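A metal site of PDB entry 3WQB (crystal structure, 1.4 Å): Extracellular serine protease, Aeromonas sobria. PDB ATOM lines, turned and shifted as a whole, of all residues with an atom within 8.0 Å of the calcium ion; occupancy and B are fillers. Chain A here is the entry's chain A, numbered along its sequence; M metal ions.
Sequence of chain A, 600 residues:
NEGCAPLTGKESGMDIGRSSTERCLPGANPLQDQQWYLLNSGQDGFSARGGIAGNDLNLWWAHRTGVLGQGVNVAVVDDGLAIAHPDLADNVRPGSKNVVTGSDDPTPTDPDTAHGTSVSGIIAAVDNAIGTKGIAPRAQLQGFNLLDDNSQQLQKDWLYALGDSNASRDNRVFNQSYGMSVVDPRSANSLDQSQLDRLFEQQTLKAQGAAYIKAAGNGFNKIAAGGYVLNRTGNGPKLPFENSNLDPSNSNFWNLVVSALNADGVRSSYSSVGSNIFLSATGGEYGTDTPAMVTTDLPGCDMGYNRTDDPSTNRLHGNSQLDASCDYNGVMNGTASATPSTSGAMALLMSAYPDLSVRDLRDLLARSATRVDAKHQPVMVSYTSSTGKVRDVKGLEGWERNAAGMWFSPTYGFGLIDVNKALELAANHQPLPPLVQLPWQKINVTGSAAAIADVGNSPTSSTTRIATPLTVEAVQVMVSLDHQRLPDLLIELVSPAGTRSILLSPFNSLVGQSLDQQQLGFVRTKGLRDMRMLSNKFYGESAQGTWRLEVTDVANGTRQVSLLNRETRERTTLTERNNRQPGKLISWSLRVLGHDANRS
SG of Cys 326 is disulfide-bonded to SG of Cys 301 (2.0 Å).
N of Gly 300 sits close to O of Ser 325.
The side-chain amide nitrogen (ND2) of Asn 306 is in hydrogen-bond range of the side-chain carboxylate (OD2) of Asp 323, 3.1 Å away.
The side-chain carboxylate (OD1) of Asp 327 is in hydrogen-bond range of the backbone NH (N) of Gly 300.
The backbone NH of Asp 297 is in hydrogen-bond range of the backbone carbonyl oxygen of Asp 327.
OD1 of Asp 297 sits at hydrogen-bond distance from ND2 of Asn 329 (3.1 Å).
O of Asp 297 lies close to NE2 of His 85.
The side-chain carboxylate of Asp 297 lies within hydrogen-bond range of the backbone NH of Tyr 305.
The nearest printed residue that does not touch the calcium ion is Pro 299 (4.1 Å).
The backbone carbonyl oxygen (O) of Met 303 is bound to the calcium ion.
O of Cys 326 binds the calcium ion, 2.4 Å away.
O of Gly 300 is bound to the calcium ion (2.4 Å).
The backbone carbonyl oxygen (O) of Leu 298 binds the calcium ion (2.4 Å).
The calcium ion is bound by the side-chain carboxylate (OD2) of Asp 297 (2.4 Å).
O of Asn 306 is bound to the calcium ion (2.5 Å).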
ATOM      1  N   HIS A  85       3.216   9.789  21.693  1.00  0.00           N
ATOM      2  CA  HIS A  85       3.706  10.111  23.031  1.00  0.00           C
ATOM      3  C   HIS A  85       4.381   8.892  23.637  1.00  0.00           C
ATOM      4  O   HIS A  85       3.821   7.792  23.585  1.00  0.00           O
ATOM      5  CB  HIS A  85       2.548  10.526  23.938  1.00  0.00           C
ATOM      6  CG  HIS A  85       2.982  11.221  25.187  1.00  0.00           C
ATOM      7  ND1 HIS A  85       3.624  10.569  26.223  1.00  0.00           N
ATOM      8  CD2 HIS A  85       2.915  12.514  25.546  1.00  0.00           C
ATOM      9  CE1 HIS A  85       3.905  11.431  27.174  1.00  0.00           C
ATOM     10  NE2 HIS A  85       3.482  12.618  26.795  1.00  0.00           N
ATOM     11  N   PRO A 111      -0.735  24.021  19.439  1.00  0.00           N
ATOM     12  CA  PRO A 111      -0.107  23.829  20.750  1.00  0.00           C
ATOM     13  C   PRO A 111      -1.062  23.748  21.948  1.00  0.00           C
ATOM     14  O   PRO A 111      -0.750  23.061  22.920  1.00  0.00           O
ATOM     15  CB  PRO A 111       0.829  25.036  20.867  1.00  0.00           C
ATOM     16  CG  PRO A 111       1.158  25.372  19.470  1.00  0.00           C
ATOM     17  CD  PRO A 111      -0.108  25.132  18.690  1.00  0.00           C
ATOM     18  N   ALA A 114      -4.361  20.193  23.815  1.00  0.00           N
ATOM     19  CA  ALA A 114      -3.732  19.169  24.655  1.00  0.00           C
ATOM     20  C   ALA A 114      -4.749  18.368  25.462  1.00  0.00           C
ATOM     21  O   ALA A 114      -4.389  17.495  26.251  1.00  0.00           O
ATOM     22  CB  ALA A 114      -2.740  19.827  25.626  1.00  0.00           C
ATOM     23  N   THR A 296      -0.267  13.026  30.922  1.00  0.00           N
ATOM     24  CA  THR A 296       0.473  13.183  29.687  1.00  0.00           C
ATOM     25  C   THR A 296       0.061  14.455  28.944  1.00  0.00           C
ATOM     26  O   THR A 296      -1.126  14.709  28.718  1.00  0.00           O
ATOM     27  CB  THR A 296       0.255  11.968  28.781  1.00  0.00           C
ATOM     28  OG1 THR A 296      -1.146  11.705  28.665  1.00  0.00           O
ATOM     29  CG2 THR A 296       0.928  10.733  29.349  1.00  0.00           C
ATOM     30  N   ASP A 297       1.057  15.231  28.544  1.00  0.00           N
ATOM     31  CA  ASP A 297       0.867  16.449  27.762  1.00  0.00           C
ATOM     32  C   ASP A 297       1.199  16.173  26.309  1.00  0.00           C
ATOM     33  O   ASP A 297       1.756  15.113  25.986  1.00  0.00           O
ATOM     34  CB  ASP A 297       1.819  17.523  28.299  1.00  0.00           C
ATOM     35  CG  ASP A 297       1.448  18.908  27.839  1.00  0.00           C
ATOM     36  OD1 ASP A 297       0.233  19.212  27.798  1.00  0.00           O
ATOM     37  OD2 ASP A 297       2.369  19.695  27.497  1.00  0.00           O
ATOM     38  N   LEU A 298       0.876  17.110  25.417  1.00  0.00           N
ATOM     39  CA  LEU A 298       1.473  17.056  24.087  1.00  0.00           C
ATOM     40  C   LEU A 298       2.993  17.056  24.234  1.00  0.00           C
ATOM     41  O   LEU A 298       3.527  17.825  25.029  1.00  0.00           O
ATOM     42  CB  LEU A 298       1.023  18.232  23.223  1.00  0.00           C
ATOM     43  CG  LEU A 298      -0.470  18.361  22.956  1.00  0.00           C
ATOM     44  CD1 LEU A 298      -0.738  19.517  22.007  1.00  0.00           C
ATOM     45  CD2 LEU A 298      -1.038  17.076  22.388  1.00  0.00           C
ATOM     46  N   PRO A 299       3.693  16.171  23.495  1.00  0.00           N
ATOM     47  CA  PRO A 299       5.137  16.065  23.718  1.00  0.00           C
ATOM     48  C   PRO A 299       5.921  17.310  23.309  1.00  0.00           C
ATOM     49  O   PRO A 299       5.546  18.001  22.361  1.00  0.00           O
ATOM     50  CB  PRO A 299       5.552  14.860  22.858  1.00  0.00           C
ATOM     51  CG  PRO A 299       4.424  14.634  21.900  1.00  0.00           C
ATOM     52  CD  PRO A 299       3.190  15.184  22.518  1.00  0.00           C
ATOM     53  N   GLY A 300       6.998  17.597  24.038  1.00  0.00           N
ATOM     54  CA  GLY A 300       7.874  18.702  23.706  1.00  0.00           C
ATOM     55  C   GLY A 300       7.517  19.975  24.427  1.00  0.00           C
ATOM     56  O   GLY A 300       6.384  20.156  24.897  1.00  0.00           O
ATOM     57  N   CYS A 301       8.483  20.867  24.535  1.00  0.00           N
ATOM     58  CA  CYS A 301       8.273  22.136  25.216  1.00  0.00           C
ATOM     59  C   CYS A 301       7.701  23.194  24.268  1.00  0.00           C
ATOM     60  O   CYS A 301       7.527  24.346  24.641  1.00  0.00           O
ATOM     61  CB  CYS A 301       9.551  22.595  25.922  1.00  0.00           C
ATOM     62  SG  CYS A 301      10.168  21.443  27.200  1.00  0.00           S
ATOM     63  N   ASP A 302       7.371  22.779  23.036  1.00  0.00           N
ATOM     64  CA  ASP A 302       6.709  23.661  22.079  1.00  0.00           C
ATOM     65  C   ASP A 302       5.219  23.362  21.884  1.00  0.00           C
ATOM     66  O   ASP A 302       4.545  24.074  21.137  1.00  0.00           O
ATOM     67  CB  ASP A 302       7.411  23.590  20.719  1.00  0.00           C
ATOM     68  CG  ASP A 302       7.479  22.175  20.166  1.00  0.00           C
ATOM     69  OD1 ASP A 302       7.357  21.190  20.942  1.00  0.00           O
ATOM     70  OD2 ASP A 302       7.648  22.041  18.938  1.00  0.00           O
ATOM     71  N   MET A 303       4.722  22.317  22.538  1.00  0.00           N
ATOM     72  CA  MET A 303       3.325  21.899  22.399  1.00  0.00           C
ATOM     73  C   MET A 303       2.754  21.553  23.760  1.00  0.00           C
ATOM     74  O   MET A 303       3.457  21.039  24.626  1.00  0.00           O
ATOM     75  CB  MET A 303       3.226  20.650  21.502  1.00  0.00           C
ATOM     76  CG  MET A 303       3.709  20.863  20.058  1.00  0.00           C
ATOM     77  SD  MET A 303       2.618  21.912  19.065  1.00  0.00           S
ATOM     78  CE  MET A 303       1.292  20.770  18.720  1.00  0.00           C
ATOM     79  N   GLY A 304       1.461  21.797  23.916  1.00  0.00           N
ATOM     80  CA  GLY A 304       0.727  21.300  25.077  1.00  0.00           C
ATOM     81  C   GLY A 304       0.525  22.319  26.173  1.00  0.00           C
ATOM     82  O   GLY A 304       0.908  23.498  26.050  1.00  0.00           O
ATOM     83  N   TYR A 305      -0.073  21.872  27.271  1.00  0.00           N
ATOM     84  CA  TYR A 305      -0.254  22.731  28.451  1.00  0.00           C
ATOM     85  C   TYR A 305       1.070  23.006  29.168  1.00  0.00           C
ATOM     86  O   TYR A 305       1.177  23.998  29.904  1.00  0.00           O
ATOM     87  CB  TYR A 305      -1.255  22.114  29.432  1.00  0.00           C
ATOM     88  CG  TYR A 305      -2.649  21.887  28.914  1.00  0.00           C
ATOM     89  CD1 TYR A 305      -3.226  22.752  27.980  1.00  0.00           C
ATOM     90  CD2 TYR A 305      -3.408  20.799  29.362  1.00  0.00           C
ATOM     91  CE1 TYR A 305      -4.518  22.547  27.519  1.00  0.00           C
ATOM     92  CE2 TYR A 305      -4.700  20.589  28.913  1.00  0.00           C
ATOM     93  CZ  TYR A 305      -5.256  21.449  27.986  1.00  0.00           C
ATOM     94  OH  TYR A 305      -6.548  21.238  27.537  1.00  0.00           O
ATOM     95  N   ASN A 306       2.052  22.137  28.963  1.00  0.00           N
ATOM     96  CA  ASN A 306       3.409  22.347  29.451  1.00  0.00           C
ATOM     97  C   ASN A 306       4.262  22.718  28.235  1.00  0.00           C
ATOM     98  O   ASN A 306       4.729  21.856  27.481  1.00  0.00           O
ATOM     99  CB  ASN A 306       3.936  21.107  30.178  1.00  0.00           C
ATOM    100  CG  ASN A 306       5.341  21.279  30.718  1.00  0.00           C
ATOM    101  OD1 ASN A 306       5.932  22.361  30.631  1.00  0.00           O
ATOM    102  ND2 ASN A 306       5.883  20.212  31.299  1.00  0.00           N
ATOM    103  N   ARG A 307       4.410  24.028  28.029  1.00  0.00           N
ATOM    104  CA  ARG A 307       5.196  24.544  26.916  1.00  0.00           C
ATOM    105  C   ARG A 307       5.772  25.903  27.293  1.00  0.00           C
ATOM    106  O   ARG A 307       5.184  26.625  28.107  1.00  0.00           O
ATOM    107  CB  ARG A 307       4.370  24.612  25.619  1.00  0.00           C
ATOM    108  CG  ARG A 307       3.295  25.672  25.583  1.00  0.00           C
ATOM    109  CD  ARG A 307       2.570  25.682  24.252  1.00  0.00           C
ATOM    110  NE  ARG A 307       1.704  26.850  24.087  1.00  0.00           N
ATOM    111  CZ  ARG A 307       0.418  26.895  24.418  1.00  0.00           C
ATOM    112  NH1 ARG A 307      -0.191  25.829  24.915  1.00  0.00           N
ATOM    113  NH2 ARG A 307      -0.289  28.005  24.236  1.00  0.00           N
ATOM    114  N   THR A 308       6.892  26.243  26.668  1.00  0.00           N
ATOM    115  CA  THR A 308       7.682  27.396  27.077  1.00  0.00           C
ATOM    116  C   THR A 308       6.899  28.704  27.052  1.00  0.00           C
ATOM    117  O   THR A 308       7.042  29.522  27.975  1.00  0.00           O
ATOM    118  CB  THR A 308       8.986  27.472  26.250  1.00  0.00           C
ATOM    119  OG1 THR A 308       9.636  26.199  26.267  1.00  0.00           O
ATOM    120  CG2 THR A 308       9.938  28.543  26.818  1.00  0.00           C
ATOM    121  N   HIS A 317       5.899  22.169  35.298  1.00  0.00           N
ATOM    122  CA  HIS A 317       6.008  22.801  33.986  1.00  0.00           C
ATOM    123  C   HIS A 317       7.345  23.509  33.805  1.00  0.00           C
ATOM    124  O   HIS A 317       7.864  24.101  34.729  1.00  0.00           O
ATOM    125  CB  HIS A 317       4.860  23.787  33.785  1.00  0.00           C
ATOM    126  CG  HIS A 317       3.519  23.130  33.632  1.00  0.00           C
ATOM    127  ND1 HIS A 317       2.629  23.530  32.660  1.00  0.00           N
ATOM    128  CD2 HIS A 317       2.912  22.131  34.322  1.00  0.00           C
ATOM    129  CE1 HIS A 317       1.528  22.790  32.751  1.00  0.00           C
ATOM    130  NE2 HIS A 317       1.682  21.938  33.750  1.00  0.00           N
ATOM    131  N   ASP A 323      10.970  17.005  34.114  1.00  0.00           N
ATOM    132  CA  ASP A 323      10.300  16.732  32.843  1.00  0.00           C
ATOM    133  C   ASP A 323      10.944  17.571  31.741  1.00  0.00           C
ATOM    134  O   ASP A 323      10.370  18.551  31.262  1.00  0.00           O
ATOM    135  CB  ASP A 323       8.795  16.992  32.974  1.00  0.00           C
ATOM    136  CG  ASP A 323       8.027  16.740  31.697  1.00  0.00           C
ATOM    137  OD1 ASP A 323       8.490  15.966  30.820  1.00  0.00           O
ATOM    138  OD2 ASP A 323       6.927  17.322  31.580  1.00  0.00           O
ATOM    139  N   SER A 325      11.614  17.230  28.558  1.00  0.00           N
ATOM    140  CA  SER A 325      10.957  17.394  27.265  1.00  0.00           C
ATOM    141  C   SER A 325       9.510  17.889  27.378  1.00  0.00           C
ATOM    142  O   SER A 325       8.800  17.902  26.382  1.00  0.00           O
ATOM    143  CB  SER A 325      10.999  16.096  26.455  1.00  0.00           C
ATOM    144  OG  SER A 325      12.313  15.871  25.981  1.00  0.00           O
ATOM    145  N   CYS A 326       9.103  18.306  28.576  1.00  0.00           N
ATOM    146  CA  CYS A 326       7.745  18.842  28.801  1.00  0.00           C
ATOM    147  C   CYS A 326       6.660  17.895  28.272  1.00  0.00           C
ATOM    148  O   CYS A 326       5.715  18.329  27.602  1.00  0.00           O
ATOM    149  CB  CYS A 326       7.590  20.221  28.145  1.00  0.00           C
ATOM    150  SG  CYS A 326       8.772  21.462  28.688  1.00  0.00           S
ATOM    151  N   ASP A 327       6.806  16.599  28.570  1.00  0.00           N
ATOM    152  CA  ASP A 327       5.888  15.585  28.091  1.00  0.00           C
ATOM    153  C   ASP A 327       4.684  15.378  29.022  1.00  0.00           C
ATOM    154  O   ASP A 327       3.785  14.608  28.682  1.00  0.00           O
ATOM    155  CB  ASP A 327       6.592  14.232  27.909  1.00  0.00           C
ATOM    156  CG  ASP A 327       7.541  14.198  26.722  1.00  0.00           C
ATOM    157  OD1 ASP A 327       7.415  15.020  25.787  1.00  0.00           O
ATOM    158  OD2 ASP A 327       8.414  13.310  26.725  1.00  0.00           O
ATOM    159  N   TYR A 328       4.689  16.047  30.179  1.00  0.00           N
ATOM    160  CA  TYR A 328       3.640  15.887  31.202  1.00  0.00           C
ATOM    161  C   TYR A 328       3.169  17.255  31.655  1.00  0.00           C
ATOM    162  O   TYR A 328       3.872  18.248  31.505  1.00  0.00           O
ATOM    163  CB  TYR A 328       4.165  15.025  32.384  1.00  0.00           C
ATOM    164  CG  TYR A 328       4.740  13.768  31.812  1.00  0.00           C
ATOM    165  CD1 TYR A 328       3.907  12.721  31.441  1.00  0.00           C
ATOM    166  CD2 TYR A 328       6.095  13.683  31.510  1.00  0.00           C
ATOM    167  CE1 TYR A 328       4.403  11.591  30.817  1.00  0.00           C
ATOM    168  CE2 TYR A 328       6.619  12.552  30.884  1.00  0.00           C
ATOM    169  CZ  TYR A 328       5.760  11.519  30.536  1.00  0.00           C
ATOM    170  OH  TYR A 328       6.242  10.400  29.915  1.00  0.00           O
ATOM    171  N   ASN A 329       1.945  17.325  32.168  1.00  0.00           N
ATOM    172  CA  ASN A 329       1.448  18.585  32.719  1.00  0.00           C
ATOM    173  C   ASN A 329       0.754  18.325  34.055  1.00  0.00           C
ATOM    174  O   ASN A 329       0.434  17.179  34.364  1.00  0.00           O
ATOM    175  CB  ASN A 329       0.544  19.342  31.713  1.00  0.00           C
ATOM    176  CG  ASN A 329      -0.852  18.721  31.561  1.00  0.00           C
ATOM    177  OD1 ASN A 329      -1.665  18.753  32.484  1.00  0.00           O
ATOM    178  ND2 ASN A 329      -1.139  18.205  30.354  1.00  0.00           N
HETATM  179 CA    CA M   1       4.418  19.739  26.203  1.00  0.00          CA
